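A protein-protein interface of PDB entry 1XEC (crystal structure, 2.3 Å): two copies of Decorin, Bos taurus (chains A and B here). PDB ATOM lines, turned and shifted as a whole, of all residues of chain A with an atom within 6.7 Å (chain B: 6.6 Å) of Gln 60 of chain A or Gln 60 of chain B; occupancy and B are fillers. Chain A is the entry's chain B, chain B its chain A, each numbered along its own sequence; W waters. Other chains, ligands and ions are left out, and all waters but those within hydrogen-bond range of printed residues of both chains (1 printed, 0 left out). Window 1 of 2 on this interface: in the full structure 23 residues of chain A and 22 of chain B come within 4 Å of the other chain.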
ATOM      1  N   GLN A  37     -11.959   7.977  22.213  1.00  0.00           N
ATOM      2  CA  GLN A  37     -12.152   8.259  20.789  1.00  0.00           C
ATOM      3  C   GLN A  37     -11.198   9.341  20.313  1.00  0.00           C
ATOM      4  O   GLN A  37     -11.359  10.518  20.629  1.00  0.00           O
ATOM      5  CB  GLN A  37     -13.613   8.679  20.549  1.00  0.00           C
ATOM      6  CG  GLN A  37     -13.997   9.077  19.114  1.00  0.00           C
ATOM      7  CD  GLN A  37     -13.630   8.033  18.087  1.00  0.00           C
ATOM      8  OE1 GLN A  37     -12.477   7.938  17.673  1.00  0.00           O
ATOM      9  NE2 GLN A  37     -14.606   7.236  17.671  1.00  0.00           N
ATOM     10  N   CYS A  38     -10.200   8.937  19.544  1.00  0.00           N
ATOM     11  CA  CYS A  38      -9.212   9.875  19.039  1.00  0.00           C
ATOM     12  C   CYS A  38      -9.071   9.840  17.526  1.00  0.00           C
ATOM     13  O   CYS A  38      -8.001  10.149  16.996  1.00  0.00           O
ATOM     14  CB  CYS A  38      -7.851   9.566  19.640  1.00  0.00           C
ATOM     15  SG  CYS A  38      -7.594   9.927  21.401  1.00  0.00           S
ATOM     16  N   SER A  39     -10.140   9.462  16.836  1.00  0.00           N
ATOM     17  CA  SER A  39     -10.128   9.390  15.377  1.00  0.00           C
ATOM     18  C   SER A  39     -10.082  10.759  14.715  1.00  0.00           C
ATOM     19  O   SER A  39     -10.478  11.751  15.313  1.00  0.00           O
ATOM     20  CB  SER A  39     -11.384   8.666  14.881  1.00  0.00           C
ATOM     21  OG  SER A  39     -11.462   7.363  15.425  1.00  0.00           O
ATOM     22  N   ASP A  40      -9.589  10.787  13.478  1.00  0.00           N
ATOM     23  CA  ASP A  40      -9.538  11.995  12.644  1.00  0.00           C
ATOM     24  C   ASP A  40      -8.863  13.234  13.224  1.00  0.00           C
ATOM     25  O   ASP A  40      -9.275  14.355  12.925  1.00  0.00           O
ATOM     26  CB  ASP A  40     -10.970  12.385  12.237  1.00  0.00           C
ATOM     27  CG  ASP A  40     -11.855  11.183  11.986  1.00  0.00           C
ATOM     28  OD1 ASP A  40     -12.842  11.010  12.722  1.00  0.00           O
ATOM     29  OD2 ASP A  40     -11.575  10.404  11.059  1.00  0.00           O
ATOM     30  N   LEU A  41      -7.819  13.052  14.023  1.00  0.00           N
ATOM     31  CA  LEU A  41      -7.171  14.200  14.639  1.00  0.00           C
ATOM     32  C   LEU A  41      -5.781  14.501  14.122  1.00  0.00           C
ATOM     33  O   LEU A  41      -5.150  15.454  14.569  1.00  0.00           O
ATOM     34  CB  LEU A  41      -7.108  14.007  16.157  1.00  0.00           C
ATOM     35  CG  LEU A  41      -8.430  13.694  16.851  1.00  0.00           C
ATOM     36  CD1 LEU A  41      -8.190  13.558  18.356  1.00  0.00           C
ATOM     37  CD2 LEU A  41      -9.437  14.804  16.559  1.00  0.00           C
ATOM     38  N   GLY A  42      -5.308  13.696  13.179  1.00  0.00           N
ATOM     39  CA  GLY A  42      -3.976  13.902  12.638  1.00  0.00           C
ATOM     40  C   GLY A  42      -2.878  13.612  13.653  1.00  0.00           C
ATOM     41  O   GLY A  42      -1.777  14.137  13.523  1.00  0.00           O
ATOM     42  N   LEU A  57      -9.927   1.615  22.455  1.00  0.00           N
ATOM     43  CA  LEU A  57      -9.145   2.767  22.047  1.00  0.00           C
ATOM     44  C   LEU A  57      -9.247   2.887  20.529  1.00  0.00           C
ATOM     45  O   LEU A  57      -8.809   1.998  19.787  1.00  0.00           O
ATOM     46  CB  LEU A  57      -7.684   2.605  22.471  1.00  0.00           C
ATOM     47  CG  LEU A  57      -6.712   3.701  22.036  1.00  0.00           C
ATOM     48  CD1 LEU A  57      -7.218   5.055  22.502  1.00  0.00           C
ATOM     49  CD2 LEU A  57      -5.324   3.417  22.603  1.00  0.00           C
ATOM     50  N   ASP A  58      -9.835   3.994  20.081  1.00  0.00           N
ATOM     51  CA  ASP A  58     -10.025   4.261  18.658  1.00  0.00           C
ATOM     52  C   ASP A  58      -9.069   5.353  18.200  1.00  0.00           C
ATOM     53  O   ASP A  58      -9.249   6.525  18.522  1.00  0.00           O
ATOM     54  CB  ASP A  58     -11.474   4.703  18.405  1.00  0.00           C
ATOM     55  CG  ASP A  58     -11.841   4.713  16.921  1.00  0.00           C
ATOM     56  OD1 ASP A  58     -10.939   4.837  16.058  1.00  0.00           O
ATOM     57  OD2 ASP A  58     -13.045   4.610  16.616  1.00  0.00           O
ATOM     58  N   LEU A  59      -8.045   4.966  17.457  1.00  0.00           N
ATOM     59  CA  LEU A  59      -7.065   5.923  16.948  1.00  0.00           C
ATOM     60  C   LEU A  59      -7.088   5.891  15.419  1.00  0.00           C
ATOM     61  O   LEU A  59      -6.079   6.106  14.745  1.00  0.00           O
ATOM     62  CB  LEU A  59      -5.677   5.570  17.482  1.00  0.00           C
ATOM     63  CG  LEU A  59      -5.504   5.880  18.977  1.00  0.00           C
ATOM     64  CD1 LEU A  59      -4.477   4.964  19.608  1.00  0.00           C
ATOM     65  CD2 LEU A  59      -5.099   7.331  19.130  1.00  0.00           C
ATOM     66  N   GLN A  60      -8.272   5.636  14.885  1.00  0.00           N
ATOM     67  CA  GLN A  60      -8.478   5.549  13.451  1.00  0.00           C
ATOM     68  C   GLN A  60      -8.248   6.859  12.709  1.00  0.00           C
ATOM     69  O   GLN A  60      -8.576   7.931  13.217  1.00  0.00           O
ATOM     70  CB  GLN A  60      -9.894   5.073  13.191  1.00  0.00           C
ATOM     71  CG  GLN A  60     -10.165   4.712  11.772  1.00  0.00           C
ATOM     72  CD  GLN A  60     -11.387   3.859  11.659  1.00  0.00           C
ATOM     73  OE1 GLN A  60     -11.667   3.307  10.605  1.00  0.00           O
ATOM     74  NE2 GLN A  60     -12.129   3.736  12.751  1.00  0.00           N
ATOM     75  N   ASN A  61      -7.691   6.756  11.504  1.00  0.00           N
ATOM     76  CA  ASN A  61      -7.421   7.906  10.633  1.00  0.00           C
ATOM     77  C   ASN A  61      -6.559   9.010  11.238  1.00  0.00           C
ATOM     78  O   ASN A  61      -6.961  10.176  11.321  1.00  0.00           O
ATOM     79  CB  ASN A  61      -8.744   8.495  10.107  1.00  0.00           C
ATOM     80  CG  ASN A  61      -8.536   9.662   9.146  1.00  0.00           C
ATOM     81  OD1 ASN A  61      -7.643   9.638   8.303  1.00  0.00           O
ATOM     82  ND2 ASN A  61      -9.373  10.680   9.263  1.00  0.00           N
ATOM     83  N   ASN A  62      -5.367   8.630  11.673  1.00  0.00           N
ATOM     84  CA  ASN A  62      -4.409   9.579  12.220  1.00  0.00           C
ATOM     85  C   ASN A  62      -3.114   9.409  11.432  1.00  0.00           C
ATOM     86  O   ASN A  62      -3.094   8.704  10.422  1.00  0.00           O
ATOM     87  CB  ASN A  62      -4.190   9.325  13.711  1.00  0.00           C
ATOM     88  CG  ASN A  62      -5.262   9.964  14.563  1.00  0.00           C
ATOM     89  OD1 ASN A  62      -5.393  11.189  14.593  1.00  0.00           O
ATOM     90  ND2 ASN A  62      -6.045   9.145  15.252  1.00  0.00           N
ATOM     91  N   ILE A  82      -7.993  -0.006  17.769  1.00  0.00           N
ATOM     92  CA  ILE A  82      -8.185   0.327  16.359  1.00  0.00           C
ATOM     93  C   ILE A  82      -7.140   1.321  15.874  1.00  0.00           C
ATOM     94  O   ILE A  82      -7.135   2.476  16.283  1.00  0.00           O
ATOM     95  CB  ILE A  82      -9.601   0.917  16.123  1.00  0.00           C
ATOM     96  CG1 ILE A  82     -10.663  -0.071  16.624  1.00  0.00           C
ATOM     97  CG2 ILE A  82      -9.817   1.188  14.638  1.00  0.00           C
ATOM     98  CD1 ILE A  82     -12.019   0.542  16.829  1.00  0.00           C
ATOM     99  N   LEU A  83      -6.258   0.868  14.994  1.00  0.00           N
ATOM    100  CA  LEU A  83      -5.194   1.716  14.463  1.00  0.00           C
ATOM    101  C   LEU A  83      -5.355   1.863  12.964  1.00  0.00           C
ATOM    102  O   LEU A  83      -4.438   2.287  12.252  1.00  0.00           O
ATOM    103  CB  LEU A  83      -3.828   1.103  14.806  1.00  0.00           C
ATOM    104  CG  LEU A  83      -3.590   1.101  16.320  1.00  0.00           C
ATOM    105  CD1 LEU A  83      -2.481   0.131  16.726  1.00  0.00           C
ATOM    106  CD2 LEU A  83      -3.261   2.516  16.736  1.00  0.00           C
ATOM    107  N   ILE A  84      -6.543   1.505  12.500  1.00  0.00           N
ATOM    108  CA  ILE A  84      -6.900   1.584  11.090  1.00  0.00           C
ATOM    109  C   ILE A  84      -6.644   2.953  10.484  1.00  0.00           C
ATOM    110  O   ILE A  84      -6.901   3.983  11.105  1.00  0.00           O
ATOM    111  CB  ILE A  84      -8.409   1.272  10.878  1.00  0.00           C
ATOM    112  CG1 ILE A  84      -8.690  -0.194  11.199  1.00  0.00           C
ATOM    113  CG2 ILE A  84      -8.832   1.623   9.450  1.00  0.00           C
ATOM    114  CD1 ILE A  84     -10.170  -0.531  11.177  1.00  0.00           C
ATOM    115  N   ASN A  85      -6.126   2.949   9.264  1.00  0.00           N
ATOM    116  CA  ASN A  85      -5.895   4.175   8.513  1.00  0.00           C
ATOM    117  C   ASN A  85      -4.904   5.165   9.123  1.00  0.00           C
ATOM    118  O   ASN A  85      -5.216   6.328   9.335  1.00  0.00           O
ATOM    119  CB  ASN A  85      -7.254   4.843   8.251  1.00  0.00           C
ATOM    120  CG  ASN A  85      -7.175   5.979   7.249  1.00  0.00           C
ATOM    121  OD1 ASN A  85      -6.516   5.879   6.219  1.00  0.00           O
ATOM    122  ND2 ASN A  85      -7.872   7.062   7.545  1.00  0.00           N
ATOM    123  N   ASN A  86      -3.700   4.677   9.392  1.00  0.00           N
ATOM    124  CA  ASN A  86      -2.609   5.492   9.922  1.00  0.00           C
ATOM    125  C   ASN A  86      -1.449   5.252   8.939  1.00  0.00           C
ATOM    126  O   ASN A  86      -1.686   4.789   7.825  1.00  0.00           O
ATOM    127  CB  ASN A  86      -2.245   5.042  11.347  1.00  0.00           C
ATOM    128  CG  ASN A  86      -3.117   5.702  12.417  1.00  0.00           C
ATOM    129  OD1 ASN A  86      -2.923   6.873  12.761  1.00  0.00           O
ATOM    130  ND2 ASN A  86      -4.090   4.958  12.934  1.00  0.00           N
ATOM    131  N   TYR A 106      -7.119  -4.141  15.104  1.00  0.00           N
ATOM    132  CA  TYR A 106      -7.329  -3.763  13.710  1.00  0.00           C
ATOM    133  C   TYR A 106      -6.197  -2.874  13.229  1.00  0.00           C
ATOM    134  O   TYR A 106      -6.091  -1.726  13.643  1.00  0.00           O
ATOM    135  CB  TYR A 106      -8.660  -3.019  13.570  1.00  0.00           C
ATOM    136  CG  TYR A 106      -9.874  -3.800  14.020  1.00  0.00           C
ATOM    137  CD1 TYR A 106     -11.120  -3.189  14.087  1.00  0.00           C
ATOM    138  CD2 TYR A 106      -9.791  -5.154  14.333  1.00  0.00           C
ATOM    139  CE1 TYR A 106     -12.268  -3.904  14.447  1.00  0.00           C
ATOM    140  CE2 TYR A 106     -10.928  -5.887  14.697  1.00  0.00           C
ATOM    141  CZ  TYR A 106     -12.169  -5.250  14.747  1.00  0.00           C
ATOM    142  OH  TYR A 106     -13.312  -5.957  15.052  1.00  0.00           O
ATOM    143  N   LYS A 109      -5.100  -0.757   6.632  1.00  0.00           N
ATOM    144  CA  LYS A 109      -4.734   0.489   5.965  1.00  0.00           C
ATOM    145  C   LYS A 109      -3.533   1.173   6.598  1.00  0.00           C
ATOM    146  O   LYS A 109      -3.609   2.308   7.078  1.00  0.00           O
ATOM    147  CB  LYS A 109      -5.911   1.461   5.917  1.00  0.00           C
ATOM    148  CG  LYS A 109      -7.008   1.049   4.960  1.00  0.00           C
ATOM    149  CD  LYS A 109      -8.033   2.159   4.830  1.00  0.00           C
ATOM    150  CE  LYS A 109      -9.206   1.748   3.961  1.00  0.00           C
ATOM    151  NZ  LYS A 109      -8.856   1.602   2.519  1.00  0.00           N
ATOM    152  N   GLN B  37     -19.648  -8.196  11.135  1.00  0.00           N
ATOM    153  CA  GLN B  37     -18.402  -7.661  10.611  1.00  0.00           C
ATOM    154  C   GLN B  37     -18.316  -7.945   9.119  1.00  0.00           C
ATOM    155  O   GLN B  37     -18.039  -9.073   8.702  1.00  0.00           O
ATOM    156  CB  GLN B  37     -17.232  -8.311  11.358  1.00  0.00           C
ATOM    157  CG  GLN B  37     -15.832  -7.906  10.896  1.00  0.00           C
ATOM    158  CD  GLN B  37     -15.660  -6.410  10.797  1.00  0.00           C
ATOM    159  OE1 GLN B  37     -16.131  -5.789   9.848  1.00  0.00           O
ATOM    160  NE2 GLN B  37     -14.998  -5.819  11.782  1.00  0.00           N
ATOM    161  N   CYS B  38     -18.564  -6.915   8.320  1.00  0.00           N
ATOM    162  CA  CYS B  38     -18.537  -7.038   6.868  1.00  0.00           C
ATOM    163  C   CYS B  38     -17.525  -6.113   6.197  1.00  0.00           C
ATOM    164  O   CYS B  38     -17.675  -5.770   5.028  1.00  0.00           O
ATOM    165  CB  CYS B  38     -19.903  -6.712   6.296  1.00  0.00           C
ATOM    166  SG  CYS B  38     -21.226  -7.961   6.377  1.00  0.00           S
ATOM    167  N   SER B  39     -16.492  -5.718   6.928  1.00  0.00           N
ATOM    168  CA  SER B  39     -15.468  -4.829   6.401  1.00  0.00           C
ATOM    169  C   SER B  39     -14.549  -5.432   5.347  1.00  0.00           C
ATOM    170  O   SER B  39     -14.385  -6.646   5.266  1.00  0.00           O
ATOM    171  CB  SER B  39     -14.603  -4.303   7.546  1.00  0.00           C
ATOM    172  OG  SER B  39     -15.403  -3.607   8.485  1.00  0.00           O
ATOM    173  N   ASP B  40     -13.961  -4.547   4.545  1.00  0.00           N
ATOM    174  CA  ASP B  40     -12.995  -4.902   3.509  1.00  0.00           C
ATOM    175  C   ASP B  40     -13.438  -5.936   2.484  1.00  0.00           C
ATOM    176  O   ASP B  40     -12.615  -6.727   2.025  1.00  0.00           O
ATOM    177  CB  ASP B  40     -11.720  -5.398   4.188  1.00  0.00           C
ATOM    178  CG  ASP B  40     -11.342  -4.553   5.392  1.00  0.00           C
ATOM    179  OD1 ASP B  40     -10.974  -5.129   6.441  1.00  0.00           O
ATOM    180  OD2 ASP B  40     -11.420  -3.315   5.290  1.00  0.00           O
ATOM    181  N   LEU B  41     -14.713  -5.923   2.103  1.00  0.00           N
ATOM    182  CA  LEU B  41     -15.200  -6.919   1.152  1.00  0.00           C
ATOM    183  C   LEU B  41     -15.624  -6.403  -0.216  1.00  0.00           C
ATOM    184  O   LEU B  41     -16.106  -7.174  -1.044  1.00  0.00           O
ATOM    185  CB  LEU B  41     -16.371  -7.698   1.763  1.00  0.00           C
ATOM    186  CG  LEU B  41     -16.079  -8.427   3.072  1.00  0.00           C
ATOM    187  CD1 LEU B  41     -17.349  -9.118   3.545  1.00  0.00           C
ATOM    188  CD2 LEU B  41     -14.953  -9.439   2.874  1.00  0.00           C
ATOM    189  N   LEU B  57     -23.102  -3.057  13.388  1.00  0.00           N
ATOM    190  CA  LEU B  57     -22.957  -3.456  11.996  1.00  0.00           C
ATOM    191  C   LEU B  57     -21.798  -2.638  11.429  1.00  0.00           C
ATOM    192  O   LEU B  57     -21.869  -1.417  11.347  1.00  0.00           O
ATOM    193  CB  LEU B  57     -24.246  -3.173  11.221  1.00  0.00           C
ATOM    194  CG  LEU B  57     -24.225  -3.300   9.686  1.00  0.00           C
ATOM    195  CD1 LEU B  57     -23.748  -4.677   9.268  1.00  0.00           C
ATOM    196  CD2 LEU B  57     -25.626  -3.040   9.136  1.00  0.00           C
ATOM    197  N   ASP B  58     -20.729  -3.333  11.061  1.00  0.00           N
ATOM    198  CA  ASP B  58     -19.525  -2.714  10.522  1.00  0.00           C
ATOM    199  C   ASP B  58     -19.445  -2.949   9.015  1.00  0.00           C
ATOM    200  O   ASP B  58     -19.165  -4.070   8.585  1.00  0.00           O
ATOM    201  CB  ASP B  58     -18.295  -3.329  11.194  1.00  0.00           C
ATOM    202  CG  ASP B  58     -17.012  -2.583  10.864  1.00  0.00           C
ATOM    203  OD1 ASP B  58     -17.043  -1.736   9.938  1.00  0.00           O
ATOM    204  OD2 ASP B  58     -15.973  -2.841  11.527  1.00  0.00           O
ATOM    205  N   LEU B  59     -19.691  -1.906   8.219  1.00  0.00           N
ATOM    206  CA  LEU B  59     -19.632  -2.019   6.758  1.00  0.00           C
ATOM    207  C   LEU B  59     -18.475  -1.185   6.213  1.00  0.00           C
ATOM    208  O   LEU B  59     -18.427  -0.811   5.041  1.00  0.00           O
ATOM    209  CB  LEU B  59     -20.956  -1.564   6.141  1.00  0.00           C
ATOM    210  CG  LEU B  59     -22.082  -2.591   6.238  1.00  0.00           C
ATOM    211  CD1 LEU B  59     -23.429  -1.908   6.091  1.00  0.00           C
ATOM    212  CD2 LEU B  59     -21.879  -3.661   5.166  1.00  0.00           C
ATOM    213  N   GLN B  60     -17.536  -0.907   7.098  1.00  0.00           N
ATOM    214  CA  GLN B  60     -16.357  -0.133   6.781  1.00  0.00           C
ATOM    215  C   GLN B  60     -15.552  -0.671   5.610  1.00  0.00           C
ATOM    216  O   GLN B  60     -15.469  -1.878   5.382  1.00  0.00           O
ATOM    217  CB  GLN B  60     -15.493  -0.072   8.019  1.00  0.00           C
ATOM    218  CG  GLN B  60     -14.172   0.559   7.845  1.00  0.00           C
ATOM    219  CD  GLN B  60     -13.691   1.116   9.139  1.00  0.00           C
ATOM    220  OE1 GLN B  60     -13.906   0.524  10.204  1.00  0.00           O
ATOM    221  NE2 GLN B  60     -13.038   2.262   9.075  1.00  0.00           N
ATOM    222  N   ASN B  61     -14.952   0.259   4.881  1.00  0.00           N
ATOM    223  CA  ASN B  61     -14.136  -0.034   3.715  1.00  0.00           C
ATOM    224  C   ASN B  61     -14.776  -0.967   2.699  1.00  0.00           C
ATOM    225  O   ASN B  61     -14.277  -2.062   2.430  1.00  0.00           O
ATOM    226  CB  ASN B  61     -12.767  -0.578   4.133  1.00  0.00           C
ATOM    227  CG  ASN B  61     -11.836  -0.801   2.942  1.00  0.00           C
ATOM    228  OD1 ASN B  61     -11.830  -0.021   1.983  1.00  0.00           O
ATOM    229  ND2 ASN B  61     -11.040  -1.855   3.005  1.00  0.00           N
ATOM    230  N   ASN B  62     -15.899  -0.532   2.141  1.00  0.00           N
ATOM    231  CA  ASN B  62     -16.568  -1.289   1.099  1.00  0.00           C
ATOM    232  C   ASN B  62     -16.771  -0.320  -0.064  1.00  0.00           C
ATOM    233  O   ASN B  62     -16.122   0.727  -0.111  1.00  0.00           O
ATOM    234  CB  ASN B  62     -17.894  -1.860   1.597  1.00  0.00           C
ATOM    235  CG  ASN B  62     -17.708  -3.164   2.346  1.00  0.00           C
ATOM    236  OD1 ASN B  62     -17.258  -4.157   1.775  1.00  0.00           O
ATOM    237  ND2 ASN B  62     -18.032  -3.166   3.629  1.00  0.00           N
ATOM    238  N   ILE B  82     -21.397   1.495  11.311  1.00  0.00           N
ATOM    239  CA  ILE B  82     -20.151   2.001  10.761  1.00  0.00           C
ATOM    240  C   ILE B  82     -20.141   1.910   9.238  1.00  0.00           C
ATOM    241  O   ILE B  82     -20.098   0.822   8.666  1.00  0.00           O
ATOM    242  CB  ILE B  82     -18.951   1.229  11.364  1.00  0.00           C
ATOM    243  CG1 ILE B  82     -18.997   1.336  12.901  1.00  0.00           C
ATOM    244  CG2 ILE B  82     -17.633   1.789  10.823  1.00  0.00           C
ATOM    245  CD1 ILE B  82     -17.924   0.519  13.621  1.00  0.00           C
ATOM    246  N   LEU B  83     -20.166   3.068   8.586  1.00  0.00           N
ATOM    247  CA  LEU B  83     -20.187   3.136   7.119  1.00  0.00           C
ATOM    248  C   LEU B  83     -18.946   3.846   6.576  1.00  0.00           C
ATOM    249  O   LEU B  83     -18.887   4.265   5.409  1.00  0.00           O
ATOM    250  CB  LEU B  83     -21.460   3.872   6.670  1.00  0.00           C
ATOM    251  CG  LEU B  83     -22.678   2.977   6.885  1.00  0.00           C
ATOM    252  CD1 LEU B  83     -23.988   3.740   6.784  1.00  0.00           C
ATOM    253  CD2 LEU B  83     -22.597   1.867   5.858  1.00  0.00           C
ATOM    254  N   ILE B  84     -17.951   3.953   7.444  1.00  0.00           N
ATOM    255  CA  ILE B  84     -16.704   4.617   7.126  1.00  0.00           C
ATOM    256  C   ILE B  84     -16.012   4.072   5.902  1.00  0.00           C
ATOM    257  O   ILE B  84     -15.966   2.864   5.668  1.00  0.00           O
ATOM    258  CB  ILE B  84     -15.730   4.527   8.316  1.00  0.00           C
ATOM    259  CG1 ILE B  84     -16.260   5.373   9.465  1.00  0.00           C
ATOM    260  CG2 ILE B  84     -14.312   4.958   7.899  1.00  0.00           C
ATOM    261  CD1 ILE B  84     -15.495   5.145  10.763  1.00  0.00           C
ATOM    262  N   ASN B  85     -15.496   4.991   5.102  1.00  0.00           N
ATOM    263  CA  ASN B  85     -14.741   4.630   3.923  1.00  0.00           C
ATOM    264  C   ASN B  85     -15.490   3.810   2.877  1.00  0.00           C
ATOM    265  O   ASN B  85     -15.111   2.685   2.543  1.00  0.00           O
ATOM    266  CB  ASN B  85     -13.465   3.916   4.380  1.00  0.00           C
ATOM    267  CG  ASN B  85     -12.528   3.597   3.246  1.00  0.00           C
ATOM    268  OD1 ASN B  85     -12.289   4.417   2.360  1.00  0.00           O
ATOM    269  ND2 ASN B  85     -11.978   2.397   3.272  1.00  0.00           N
ATOM    270  N   ASN B  86     -16.579   4.378   2.380  1.00  0.00           N
ATOM    271  CA  ASN B  86     -17.350   3.752   1.317  1.00  0.00           C
ATOM    272  C   ASN B  86     -17.402   4.799   0.206  1.00  0.00           C
ATOM    273  O   ASN B  86     -16.493   5.630   0.104  1.00  0.00           O
ATOM    274  CB  ASN B  86     -18.751   3.380   1.809  1.00  0.00           C
ATOM    275  CG  ASN B  86     -18.774   2.032   2.516  1.00  0.00           C
ATOM    276  OD1 ASN B  86     -18.852   0.976   1.878  1.00  0.00           O
ATOM    277  ND2 ASN B  86     -18.684   2.064   3.839  1.00  0.00           N
ATOM    278  N   TYR B 106     -21.399   6.488  12.035  1.00  0.00           N
ATOM    279  CA  TYR B 106     -20.111   6.893  11.479  1.00  0.00           C
ATOM    280  C   TYR B 106     -20.156   6.858   9.957  1.00  0.00           C
ATOM    281  O   TYR B 106     -20.206   5.776   9.370  1.00  0.00           O
ATOM    282  CB  TYR B 106     -19.003   5.949  11.984  1.00  0.00           C
ATOM    283  CG  TYR B 106     -18.825   5.919  13.491  1.00  0.00           C
ATOM    284  CD1 TYR B 106     -17.991   4.975  14.094  1.00  0.00           C
ATOM    285  CD2 TYR B 106     -19.448   6.865  14.314  1.00  0.00           C
ATOM    286  CE1 TYR B 106     -17.779   4.973  15.486  1.00  0.00           C
ATOM    287  CE2 TYR B 106     -19.237   6.880  15.692  1.00  0.00           C
ATOM    288  CZ  TYR B 106     -18.398   5.930  16.272  1.00  0.00           C
ATOM    289  OH  TYR B 106     -18.162   5.962  17.627  1.00  0.00           O
HETATM  290  O   HOH W   1     -13.574   1.585  12.979  1.00  0.00           O
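The backbone NH (N) of Gln 60 of chain B is in hydrogen-bond range of the backbone carbonyl oxygen (O) of Ile 82 of chain B (3.5 Å).
OD2 of Asp 40 of chain B is in hydrogen-bond range of ND2 of Asn 61 of chain B (2.7 Å).
OD1 of Asp 58 of chain B sits close to N of Gln 60 of chain B (3.0 Å).
The side-chain amide nitrogen of Asn 62 of chain A is in hydrogen-bond range of the backbone carbonyl oxygen of Gln 60 of chain A (3.5 Å).
The side-chain amide nitrogen (NE2) of Gln 37 of chain A is in hydrogen-bond range of the side-chain carboxylate (OD2) of Asp 58 of chain A (3.2 Å).
O of Gln 60 of chain A is in hydrogen-bond range of N of Asp 40 of chain A, 3.0 Å away.
Gln 37 of chain A touches Tyr 106 of chain B, and with the chains exchanged Tyr 106 of chain A touches Gln 37 of chain B.
Gln 60 of chain B touches its own counterpart, Gln 60 of chain A.
Of the 5 pairs that touch across the chains among the printed residues, 3 have their exchanged pair printed and touching as well.
Among the printed residues, pairs that only touch across the chains: Gln 37 of chain A with Tyr 106 of chain B and Tyr 106 of chain A with Gln 37 of chain B.
Water W1 lies within hydrogen-bond range of the side-chain amide nitrogen of Gln 60 of chain A and the side-chain amide oxygen of Gln 60 of chain B.
Printed residues of chain B within 4 Å of Gln 37 of chain A: Tyr 106.
Ser 39 of chain A touches none of the printed residues of chain B.
Printed residues of chain B within 4 Å of Tyr 106 of chain A: Gln 37 (3.7 Å).
Printed residues of chain B within 4 Å of Lys 109 of chain A: Asn 61 (3.4 Å) and Asn 85 (2.9 Å).
Leu 59 of chain B touches none of the printed residues of chain A.
Of the printed residues of chain A, Gln 60 of chain B touches Gln 60 (2.3 Å).
Of the printed residues of chain A, Asn 61 of chain B touches Lys 109 (3.4 Å).
The nearest printed residue of chain A that does not touch Gln 60 of chain B is Ile 84 of chain A (4.002 Å).
The side-chain amide oxygen (OD1) of Asn 61 of chain B is in hydrogen-bond range of the side-chain amino group (NZ) of Lys 109 of chain A (3.4 Å).
The side-chain amide oxygen (OE1) of Gln 60 of chain A lies close to the side-chain amide nitrogen (NE2) of Gln 60 of chain B (2.3 Å).
The side-chain amide nitrogen of Asn 85 of chain B lies close to the side-chain amino group of Lys 109 of chain A.
Of the 19 printed residues of chain A, 4 touch a printed residue of chain B.
Of the 17 printed residues of chain B, 5 touch a printed residue of chain A.
Among the printed residues, no Asp or Glu carboxylate lies within 4 Å of a Lys or Arg side-chain nitrogen of the other chain.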
